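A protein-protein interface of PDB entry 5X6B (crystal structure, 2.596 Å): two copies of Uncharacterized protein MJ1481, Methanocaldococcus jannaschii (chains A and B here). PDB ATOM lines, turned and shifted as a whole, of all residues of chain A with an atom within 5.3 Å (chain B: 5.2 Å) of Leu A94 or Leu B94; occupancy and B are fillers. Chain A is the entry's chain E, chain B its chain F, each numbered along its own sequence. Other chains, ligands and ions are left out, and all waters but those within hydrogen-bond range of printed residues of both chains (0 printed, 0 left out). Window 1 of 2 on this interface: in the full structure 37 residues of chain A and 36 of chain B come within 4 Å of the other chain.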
ATOM      1  N   ALA A  55      18.685  -4.392  14.908  1.00  0.00           N
ATOM      2  CA  ALA A  55      18.184  -5.197  16.016  1.00  0.00           C
ATOM      3  C   ALA A  55      18.009  -6.656  15.618  1.00  0.00           C
ATOM      4  O   ALA A  55      18.445  -7.562  16.325  1.00  0.00           O
ATOM      5  CB  ALA A  55      16.875  -4.634  16.518  1.00  0.00           C
ATOM      6  N   LEU A  59      20.032 -10.547  16.393  1.00  0.00           N
ATOM      7  CA  LEU A  59      19.403 -11.776  16.856  1.00  0.00           C
ATOM      8  C   LEU A  59      19.687 -12.897  15.873  1.00  0.00           C
ATOM      9  O   LEU A  59      19.720 -14.071  16.239  1.00  0.00           O
ATOM     10  CB  LEU A  59      17.899 -11.589  17.038  1.00  0.00           C
ATOM     11  CG  LEU A  59      17.493 -10.668  18.188  1.00  0.00           C
ATOM     12  CD1 LEU A  59      15.995 -10.765  18.429  1.00  0.00           C
ATOM     13  CD2 LEU A  59      18.267 -11.003  19.462  1.00  0.00           C
ATOM     14  N   ILE A  87      22.834  -9.857  22.399  1.00  0.00           N
ATOM     15  CA  ILE A  87      21.515  -9.636  22.977  1.00  0.00           C
ATOM     16  C   ILE A  87      21.347  -8.221  23.521  1.00  0.00           C
ATOM     17  O   ILE A  87      20.326  -7.575  23.290  1.00  0.00           O
ATOM     18  CB  ILE A  87      21.235 -10.633  24.108  1.00  0.00           C
ATOM     19  CG1 ILE A  87      21.430 -12.064  23.607  1.00  0.00           C
ATOM     20  CG2 ILE A  87      19.831 -10.436  24.666  1.00  0.00           C
ATOM     21  CD1 ILE A  87      20.510 -12.436  22.471  1.00  0.00           C
ATOM     22  N   LYS A  89      23.182  -5.445  22.804  1.00  0.00           N
ATOM     23  CA  LYS A  89      23.228  -4.492  21.698  1.00  0.00           C
ATOM     24  C   LYS A  89      21.893  -4.454  20.940  1.00  0.00           C
ATOM     25  O   LYS A  89      21.480  -3.404  20.447  1.00  0.00           O
ATOM     26  CB  LYS A  89      24.378  -4.831  20.741  1.00  0.00           C
ATOM     27  CG  LYS A  89      25.582  -3.908  20.880  1.00  0.00           C
ATOM     28  CD  LYS A  89      26.741  -4.335  19.986  1.00  0.00           C
ATOM     29  CE  LYS A  89      26.647  -3.670  18.621  1.00  0.00           C
ATOM     30  NZ  LYS A  89      26.723  -2.180  18.712  1.00  0.00           N
ATOM     31  N   CYS A  90      21.218  -5.599  20.855  1.00  0.00           N
ATOM     32  CA  CYS A  90      19.885  -5.639  20.266  1.00  0.00           C
ATOM     33  C   CYS A  90      18.931  -4.775  21.097  1.00  0.00           C
ATOM     34  O   CYS A  90      18.205  -3.942  20.552  1.00  0.00           O
ATOM     35  CB  CYS A  90      19.378  -7.082  20.164  1.00  0.00           C
ATOM     36  SG  CYS A  90      17.683  -7.266  19.581  1.00  0.00           S
ATOM     37  N   GLN A  91      18.959  -4.955  22.415  1.00  0.00           N
ATOM     38  CA  GLN A  91      18.105  -4.184  23.319  1.00  0.00           C
ATOM     39  C   GLN A  91      18.344  -2.681  23.264  1.00  0.00           C
ATOM     40  O   GLN A  91      17.420  -1.899  23.474  1.00  0.00           O
ATOM     41  CB  GLN A  91      18.280  -4.670  24.757  1.00  0.00           C
ATOM     42  CG  GLN A  91      17.514  -5.942  25.019  1.00  0.00           C
ATOM     43  CD  GLN A  91      17.620  -6.402  26.442  1.00  0.00           C
ATOM     44  OE1 GLN A  91      18.610  -6.130  27.120  1.00  0.00           O
ATOM     45  NE2 GLN A  91      16.595  -7.103  26.917  1.00  0.00           N
ATOM     46  N   GLU A  92      19.574  -2.274  22.980  1.00  0.00           N
ATOM     47  CA  GLU A  92      19.862  -0.850  22.865  1.00  0.00           C
ATOM     48  C   GLU A  92      19.289  -0.286  21.574  1.00  0.00           C
ATOM     49  O   GLU A  92      18.842   0.862  21.531  1.00  0.00           O
ATOM     50  CB  GLU A  92      21.364  -0.587  22.956  1.00  0.00           C
ATOM     51  CG  GLU A  92      22.032  -1.377  24.068  1.00  0.00           C
ATOM     52  CD  GLU A  92      23.540  -1.200  24.119  1.00  0.00           C
ATOM     53  OE1 GLU A  92      24.153  -0.920  23.063  1.00  0.00           O
ATOM     54  OE2 GLU A  92      24.111  -1.360  25.221  1.00  0.00           O
ATOM     55  N   HIS A  93      19.279  -1.100  20.525  1.00  0.00           N
ATOM     56  CA  HIS A  93      18.670  -0.690  19.268  1.00  0.00           C
ATOM     57  C   HIS A  93      17.157  -0.623  19.423  1.00  0.00           C
ATOM     58  O   HIS A  93      16.505   0.255  18.861  1.00  0.00           O
ATOM     59  CB  HIS A  93      19.049  -1.646  18.139  1.00  0.00           C
ATOM     60  CG  HIS A  93      20.457  -1.483  17.656  1.00  0.00           C
ATOM     61  ND1 HIS A  93      20.959  -0.274  17.230  1.00  0.00           N
ATOM     62  CD2 HIS A  93      21.465  -2.375  17.527  1.00  0.00           C
ATOM     63  CE1 HIS A  93      22.218  -0.425  16.859  1.00  0.00           C
ATOM     64  NE2 HIS A  93      22.550  -1.694  17.028  1.00  0.00           N
ATOM     65  N   LEU A  94      16.605  -1.554  20.194  1.00  0.00           N
ATOM     66  CA  LEU A  94      15.171  -1.582  20.431  1.00  0.00           C
ATOM     67  C   LEU A  94      14.737  -0.377  21.267  1.00  0.00           C
ATOM     68  O   LEU A  94      13.678   0.206  21.022  1.00  0.00           O
ATOM     69  CB  LEU A  94      14.762  -2.888  21.114  1.00  0.00           C
ATOM     70  CG  LEU A  94      14.963  -4.165  20.290  1.00  0.00           C
ATOM     71  CD1 LEU A  94      14.499  -5.392  21.057  1.00  0.00           C
ATOM     72  CD2 LEU A  94      14.244  -4.061  18.955  1.00  0.00           C
ATOM     73  N   ASN A  95      15.555   0.003  22.242  1.00  0.00           N
ATOM     74  CA  ASN A  95      15.253   1.179  23.049  1.00  0.00           C
ATOM     75  C   ASN A  95      15.249   2.454  22.205  1.00  0.00           C
ATOM     76  O   ASN A  95      14.411   3.328  22.407  1.00  0.00           O
ATOM     77  CB  ASN A  95      16.239   1.316  24.211  1.00  0.00           C
ATOM     78  CG  ASN A  95      15.930   0.364  25.359  1.00  0.00           C
ATOM     79  OD1 ASN A  95      14.821  -0.160  25.469  1.00  0.00           O
ATOM     80  ND2 ASN A  95      16.909   0.153  26.232  1.00  0.00           N
ATOM     81  N   LYS A  96      16.173   2.551  21.253  1.00  0.00           N
ATOM     82  CA  LYS A  96      16.210   3.702  20.353  1.00  0.00           C
ATOM     83  C   LYS A  96      14.943   3.773  19.501  1.00  0.00           C
ATOM     84  O   LYS A  96      14.458   4.859  19.178  1.00  0.00           O
ATOM     85  CB  LYS A  96      17.440   3.651  19.443  1.00  0.00           C
ATOM     86  CG  LYS A  96      18.761   3.797  20.169  1.00  0.00           C
ATOM     87  CD  LYS A  96      19.902   3.948  19.182  1.00  0.00           C
ATOM     88  CE  LYS A  96      21.251   3.963  19.880  1.00  0.00           C
ATOM     89  NZ  LYS A  96      22.370   4.003  18.897  1.00  0.00           N
ATOM     90  N   ILE A  97      14.418   2.608  19.136  1.00  0.00           N
ATOM     91  CA  ILE A  97      13.153   2.528  18.420  1.00  0.00           C
ATOM     92  C   ILE A  97      12.017   3.038  19.300  1.00  0.00           C
ATOM     93  O   ILE A  97      11.190   3.837  18.863  1.00  0.00           O
ATOM     94  CB  ILE A  97      12.845   1.088  17.973  1.00  0.00           C
ATOM     95  CG1 ILE A  97      13.871   0.620  16.939  1.00  0.00           C
ATOM     96  CG2 ILE A  97      11.434   0.989  17.421  1.00  0.00           C
ATOM     97  CD1 ILE A  97      13.745  -0.835  16.589  1.00  0.00           C
ATOM     98  N   LEU A  98      11.991   2.569  20.544  1.00  0.00           N
ATOM     99  CA  LEU A  98      10.976   2.979  21.506  1.00  0.00           C
ATOM    100  C   LEU A  98      11.088   4.457  21.887  1.00  0.00           C
ATOM    101  O   LEU A  98      10.124   5.057  22.357  1.00  0.00           O
ATOM    102  CB  LEU A  98      11.063   2.112  22.761  1.00  0.00           C
ATOM    103  CG  LEU A  98      10.657   0.654  22.573  1.00  0.00           C
ATOM    104  CD1 LEU A  98      10.704  -0.105  23.896  1.00  0.00           C
ATOM    105  CD2 LEU A  98       9.269   0.578  21.954  1.00  0.00           C
ATOM    106  N   ALA A  99      12.266   5.036  21.684  1.00  0.00           N
ATOM    107  CA  ALA A  99      12.482   6.445  21.980  1.00  0.00           C
ATOM    108  C   ALA A  99      11.622   7.329  21.081  1.00  0.00           C
ATOM    109  O   ALA A  99      11.180   8.404  21.490  1.00  0.00           O
ATOM    110  CB  ALA A  99      13.958   6.801  21.826  1.00  0.00           C
ATOM    111  N   ALA B  55      11.240 -14.320  21.267  1.00  0.00           N
ATOM    112  CA  ALA B  55      11.806 -12.999  21.002  1.00  0.00           C
ATOM    113  C   ALA B  55      11.887 -12.704  19.514  1.00  0.00           C
ATOM    114  O   ALA B  55      11.486 -11.633  19.061  1.00  0.00           O
ATOM    115  CB  ALA B  55      13.188 -12.875  21.626  1.00  0.00           C
ATOM    116  N   LEU B  59       9.758  -9.884  16.798  1.00  0.00           N
ATOM    117  CA  LEU B  59      10.326  -8.951  15.823  1.00  0.00           C
ATOM    118  C   LEU B  59       9.853  -9.271  14.407  1.00  0.00           C
ATOM    119  O   LEU B  59       9.676  -8.370  13.584  1.00  0.00           O
ATOM    120  CB  LEU B  59      11.857  -8.959  15.870  1.00  0.00           C
ATOM    121  CG  LEU B  59      12.501  -8.182  17.020  1.00  0.00           C
ATOM    122  CD1 LEU B  59      14.012  -8.023  16.817  1.00  0.00           C
ATOM    123  CD2 LEU B  59      11.838  -6.827  17.152  1.00  0.00           C
ATOM    124  N   ILE B  87       7.657  -4.862  20.413  1.00  0.00           N
ATOM    125  CA  ILE B  87       9.022  -4.542  20.818  1.00  0.00           C
ATOM    126  C   ILE B  87       9.265  -4.754  22.314  1.00  0.00           C
ATOM    127  O   ILE B  87      10.296  -5.294  22.711  1.00  0.00           O
ATOM    128  CB  ILE B  87       9.369  -3.091  20.466  1.00  0.00           C
ATOM    129  CG1 ILE B  87       9.097  -2.837  18.983  1.00  0.00           C
ATOM    130  CG2 ILE B  87      10.819  -2.781  20.824  1.00  0.00           C
ATOM    131  CD1 ILE B  87       9.936  -3.684  18.060  1.00  0.00           C
ATOM    132  N   CYS B  90       9.227  -8.337  23.382  1.00  0.00           N
ATOM    133  CA  CYS B  90      10.466  -8.939  22.913  1.00  0.00           C
ATOM    134  C   CYS B  90      11.618  -8.659  23.876  1.00  0.00           C
ATOM    135  O   CYS B  90      12.387  -9.562  24.224  1.00  0.00           O
ATOM    136  CB  CYS B  90      10.806  -8.425  21.517  1.00  0.00           C
ATOM    137  SG  CYS B  90      12.460  -8.852  20.942  1.00  0.00           S
ATOM    138  N   GLN B  91      11.727  -7.405  24.304  1.00  0.00           N
ATOM    139  CA  GLN B  91      12.768  -7.003  25.245  1.00  0.00           C
ATOM    140  C   GLN B  91      12.633  -7.719  26.580  1.00  0.00           C
ATOM    141  O   GLN B  91      13.619  -7.915  27.291  1.00  0.00           O
ATOM    142  CB  GLN B  91      12.741  -5.493  25.464  1.00  0.00           C
ATOM    143  CG  GLN B  91      13.713  -4.742  24.576  1.00  0.00           C
ATOM    144  CD  GLN B  91      13.596  -3.242  24.734  1.00  0.00           C
ATOM    145  OE1 GLN B  91      12.596  -2.738  25.246  1.00  0.00           O
ATOM    146  NE2 GLN B  91      14.625  -2.518  24.303  1.00  0.00           N
ATOM    147  N   GLU B  92      11.412  -8.116  26.919  1.00  0.00           N
ATOM    148  CA  GLU B  92      11.204  -8.874  28.141  1.00  0.00           C
ATOM    149  C   GLU B  92      11.758 -10.285  27.994  1.00  0.00           C
ATOM    150  O   GLU B  92      12.417 -10.802  28.897  1.00  0.00           O
ATOM    151  CB  GLU B  92       9.721  -8.919  28.514  1.00  0.00           C
ATOM    152  CG  GLU B  92       9.430  -9.750  29.754  1.00  0.00           C
ATOM    153  CD  GLU B  92      10.261  -9.329  30.954  1.00  0.00           C
ATOM    154  OE1 GLU B  92      10.598  -8.128  31.068  1.00  0.00           O
ATOM    155  OE2 GLU B  92      10.586 -10.208  31.781  1.00  0.00           O
ATOM    156  N   HIS B  93      11.496 -10.898  26.847  1.00  0.00           N
ATOM    157  CA  HIS B  93      11.984 -12.242  26.576  1.00  0.00           C
ATOM    158  C   HIS B  93      13.507 -12.252  26.517  1.00  0.00           C
ATOM    159  O   HIS B  93      14.148 -13.173  27.020  1.00  0.00           O
ATOM    160  CB  HIS B  93      11.386 -12.775  25.276  1.00  0.00           C
ATOM    161  CG  HIS B  93       9.937 -13.131  25.382  1.00  0.00           C
ATOM    162  ND1 HIS B  93       9.464 -14.061  26.285  1.00  0.00           N
ATOM    163  CD2 HIS B  93       8.855 -12.689  24.700  1.00  0.00           C
ATOM    164  CE1 HIS B  93       8.155 -14.174  26.154  1.00  0.00           C
ATOM    165  NE2 HIS B  93       7.759 -13.352  25.199  1.00  0.00           N
ATOM    166  N   LEU B  94      14.079 -11.216  25.915  1.00  0.00           N
ATOM    167  CA  LEU B  94      15.526 -11.045  25.897  1.00  0.00           C
ATOM    168  C   LEU B  94      16.081 -10.936  27.320  1.00  0.00           C
ATOM    169  O   LEU B  94      17.150 -11.475  27.617  1.00  0.00           O
ATOM    170  CB  LEU B  94      15.913  -9.808  25.084  1.00  0.00           C
ATOM    171  CG  LEU B  94      15.601  -9.854  23.587  1.00  0.00           C
ATOM    172  CD1 LEU B  94      15.992  -8.545  22.913  1.00  0.00           C
ATOM    173  CD2 LEU B  94      16.303 -11.037  22.928  1.00  0.00           C
ATOM    174  N   ASN B  95      15.349 -10.250  28.198  1.00  0.00           N
ATOM    175  CA  ASN B  95      15.761 -10.111  29.592  1.00  0.00           C
ATOM    176  C   ASN B  95      15.721 -11.437  30.350  1.00  0.00           C
ATOM    177  O   ASN B  95      16.529 -11.660  31.248  1.00  0.00           O
ATOM    178  CB  ASN B  95      14.893  -9.078  30.320  1.00  0.00           C
ATOM    179  CG  ASN B  95      15.318  -7.646  30.035  1.00  0.00           C
ATOM    180  OD1 ASN B  95      16.456  -7.387  29.646  1.00  0.00           O
ATOM    181  ND2 ASN B  95      14.398  -6.709  30.227  1.00  0.00           N
ATOM    182  N   LYS B  96      14.782 -12.314  30.003  1.00  0.00           N
ATOM    183  CA  LYS B  96      14.737 -13.628  30.636  1.00  0.00           C
ATOM    184  C   LYS B  96      15.937 -14.465  30.209  1.00  0.00           C
ATOM    185  O   LYS B  96      16.461 -15.261  30.988  1.00  0.00           O
ATOM    186  CB  LYS B  96      13.437 -14.360  30.302  1.00  0.00           C
ATOM    187  CG  LYS B  96      12.211 -13.782  30.988  1.00  0.00           C
ATOM    188  CD  LYS B  96      10.986 -14.641  30.744  1.00  0.00           C
ATOM    189  CE  LYS B  96       9.730 -13.982  31.286  1.00  0.00           C
ATOM    190  NZ  LYS B  96       8.503 -14.700  30.840  1.00  0.00           N
ATOM    191  N   ILE B  97      16.369 -14.270  28.967  1.00  0.00           N
ATOM    192  CA  ILE B  97      17.549 -14.948  28.450  1.00  0.00           C
ATOM    193  C   ILE B  97      18.811 -14.473  29.173  1.00  0.00           C
ATOM    194  O   ILE B  97      19.635 -15.284  29.595  1.00  0.00           O
ATOM    195  CB  ILE B  97      17.702 -14.720  26.937  1.00  0.00           C
ATOM    196  CG1 ILE B  97      16.483 -15.272  26.193  1.00  0.00           C
ATOM    197  CG2 ILE B  97      18.980 -15.363  26.415  1.00  0.00           C
ATOM    198  CD1 ILE B  97      16.485 -14.949  24.717  1.00  0.00           C
ATOM    199  N   LEU B  98      18.942 -13.158  29.327  1.00  0.00           N
ATOM    200  CA  LEU B  98      20.085 -12.560  30.016  1.00  0.00           C
ATOM    201  C   LEU B  98      20.139 -12.943  31.495  1.00  0.00           C
ATOM    202  O   LEU B  98      21.202 -12.913  32.111  1.00  0.00           O
ATOM    203  CB  LEU B  98      20.051 -11.033  29.884  1.00  0.00           C
ATOM    204  CG  LEU B  98      20.409 -10.426  28.525  1.00  0.00           C
ATOM    205  CD1 LEU B  98      20.267  -8.913  28.558  1.00  0.00           C
ATOM    206  CD2 LEU B  98      21.814 -10.820  28.100  1.00  0.00           C
ATOM    207  N   ALA B  99      18.991 -13.299  32.060  1.00  0.00           N
ATOM    208  CA  ALA B  99      18.928 -13.684  33.464  1.00  0.00           C
ATOM    209  C   ALA B  99      19.677 -14.987  33.691  1.00  0.00           C
ATOM    210  O   ALA B  99      20.169 -15.246  34.789  1.00  0.00           O
ATOM    211  CB  ALA B  99      17.485 -13.813  33.919  1.00  0.00           C
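NE2 of Gln B91 is in hydrogen-bond range of O of Gln A91, 3.0 Å away.
The side-chain amide oxygen of Asn A95 sits at hydrogen-bond distance from the side-chain amide nitrogen of Gln B91, at 2.6 Å.
OD1 of Asn B95 is in hydrogen-bond range of NE2 of Gln A91 (2.7 Å).
SG of Cys A90 sits at hydrogen-bond distance from O of Ala A55 (3.4 Å).
O of Gln A91 sits close to ND2 of Asn A95 (3.5 Å).
O of Gln B91 sits close to ND2 of Asn B95 (3.3 Å).
Leu B94 touches Leu A59.
Ile A87 touches Leu B94 (CG2 to CD2, 3.98 Å).
CG2 of Ile A87 touches CG of Leu B98, 3.9 Å away.
Gln A91 touches Leu B94.
OE1 of Gln A91 touches CD1 of Leu B98 (3.5 Å).
CG2 of Ile B87 touches CB of Leu A94 (3.96 Å).
NE2 of Gln B91 touches CB of Leu A94, 3.2 Å away.
Leu B94 touches Leu A94.
CG of Leu A98 touches CG2 of Ile B87 (3.9 Å).
CD1 of Leu A98 touches OE1 of Gln B91, at 3.5 Å.
Of the printed residues of chain B, Leu A59 touches Leu B59 (3.7 Å) and Leu B94 (3.98 Å).
Printed residues of chain B within 4 Å of Gln A91: Gln B91 (3.0 Å), Leu B94 (3.3 Å), Asn B95 (2.7 Å) and Leu B98 (3.5 Å).
Of the printed residues of chain B, Leu A94 touches Ile B87 (3.96 Å), Gln B91 (3.2 Å) and Leu B94 (3.95 Å).
Of the printed residues of chain B, Leu A98 touches Ile B87 and Gln B91.
Cys B90 touches none of the printed residues of chain A.
Of the printed residues of chain A, Gln B91 touches Gln A91 (3.0 Å), Leu A94 (3.2 Å), Asn A95 (2.6 Å) and Leu A98 (3.5 Å).
Of the printed residues of chain A, Leu B94 touches Leu A59 (3.98 Å), Ile A87 (3.98 Å), Cys A90 (3.9 Å), Gln A91 (3.3 Å) and Leu A94 (3.95 Å).
Of the printed residues of chain A, Asn B95 touches Gln A91 (2.7 Å).
The nearest printed residue of chain B that does not touch Leu A94 is Cys B90 (4.02 Å).
Hydrophobic or aromatic side chains of chain A within 4 Å of the printed part of chain B: Leu A59, Ile A87, Leu A94 and Leu A98.
Of the 13 printed residues of chain B, 6 touch a printed residue of chain A.
Among the printed residues, 15 pairs touch across the chains.
Among the printed residues, no Asp or Glu carboxylate lies within 4 Å of a Lys or Arg side-chain nitrogen of the other chain.
Ile A87 touches Leu B94, and with the chains exchanged Leu A94 touches Ile B87.
Gln A91 touches Asn B95, and with the chains exchanged Asn A95 touches Gln B91.
Gln A91 touches Leu B98, and with the chains exchanged Leu A98 touches Gln B91.
Leu B94 touches its own counterpart, Leu A94.
Positions printed for both chains: 55, 59, 87, 90, 91, 92, 93, 94, 95, 96, 97, 98 and 99.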
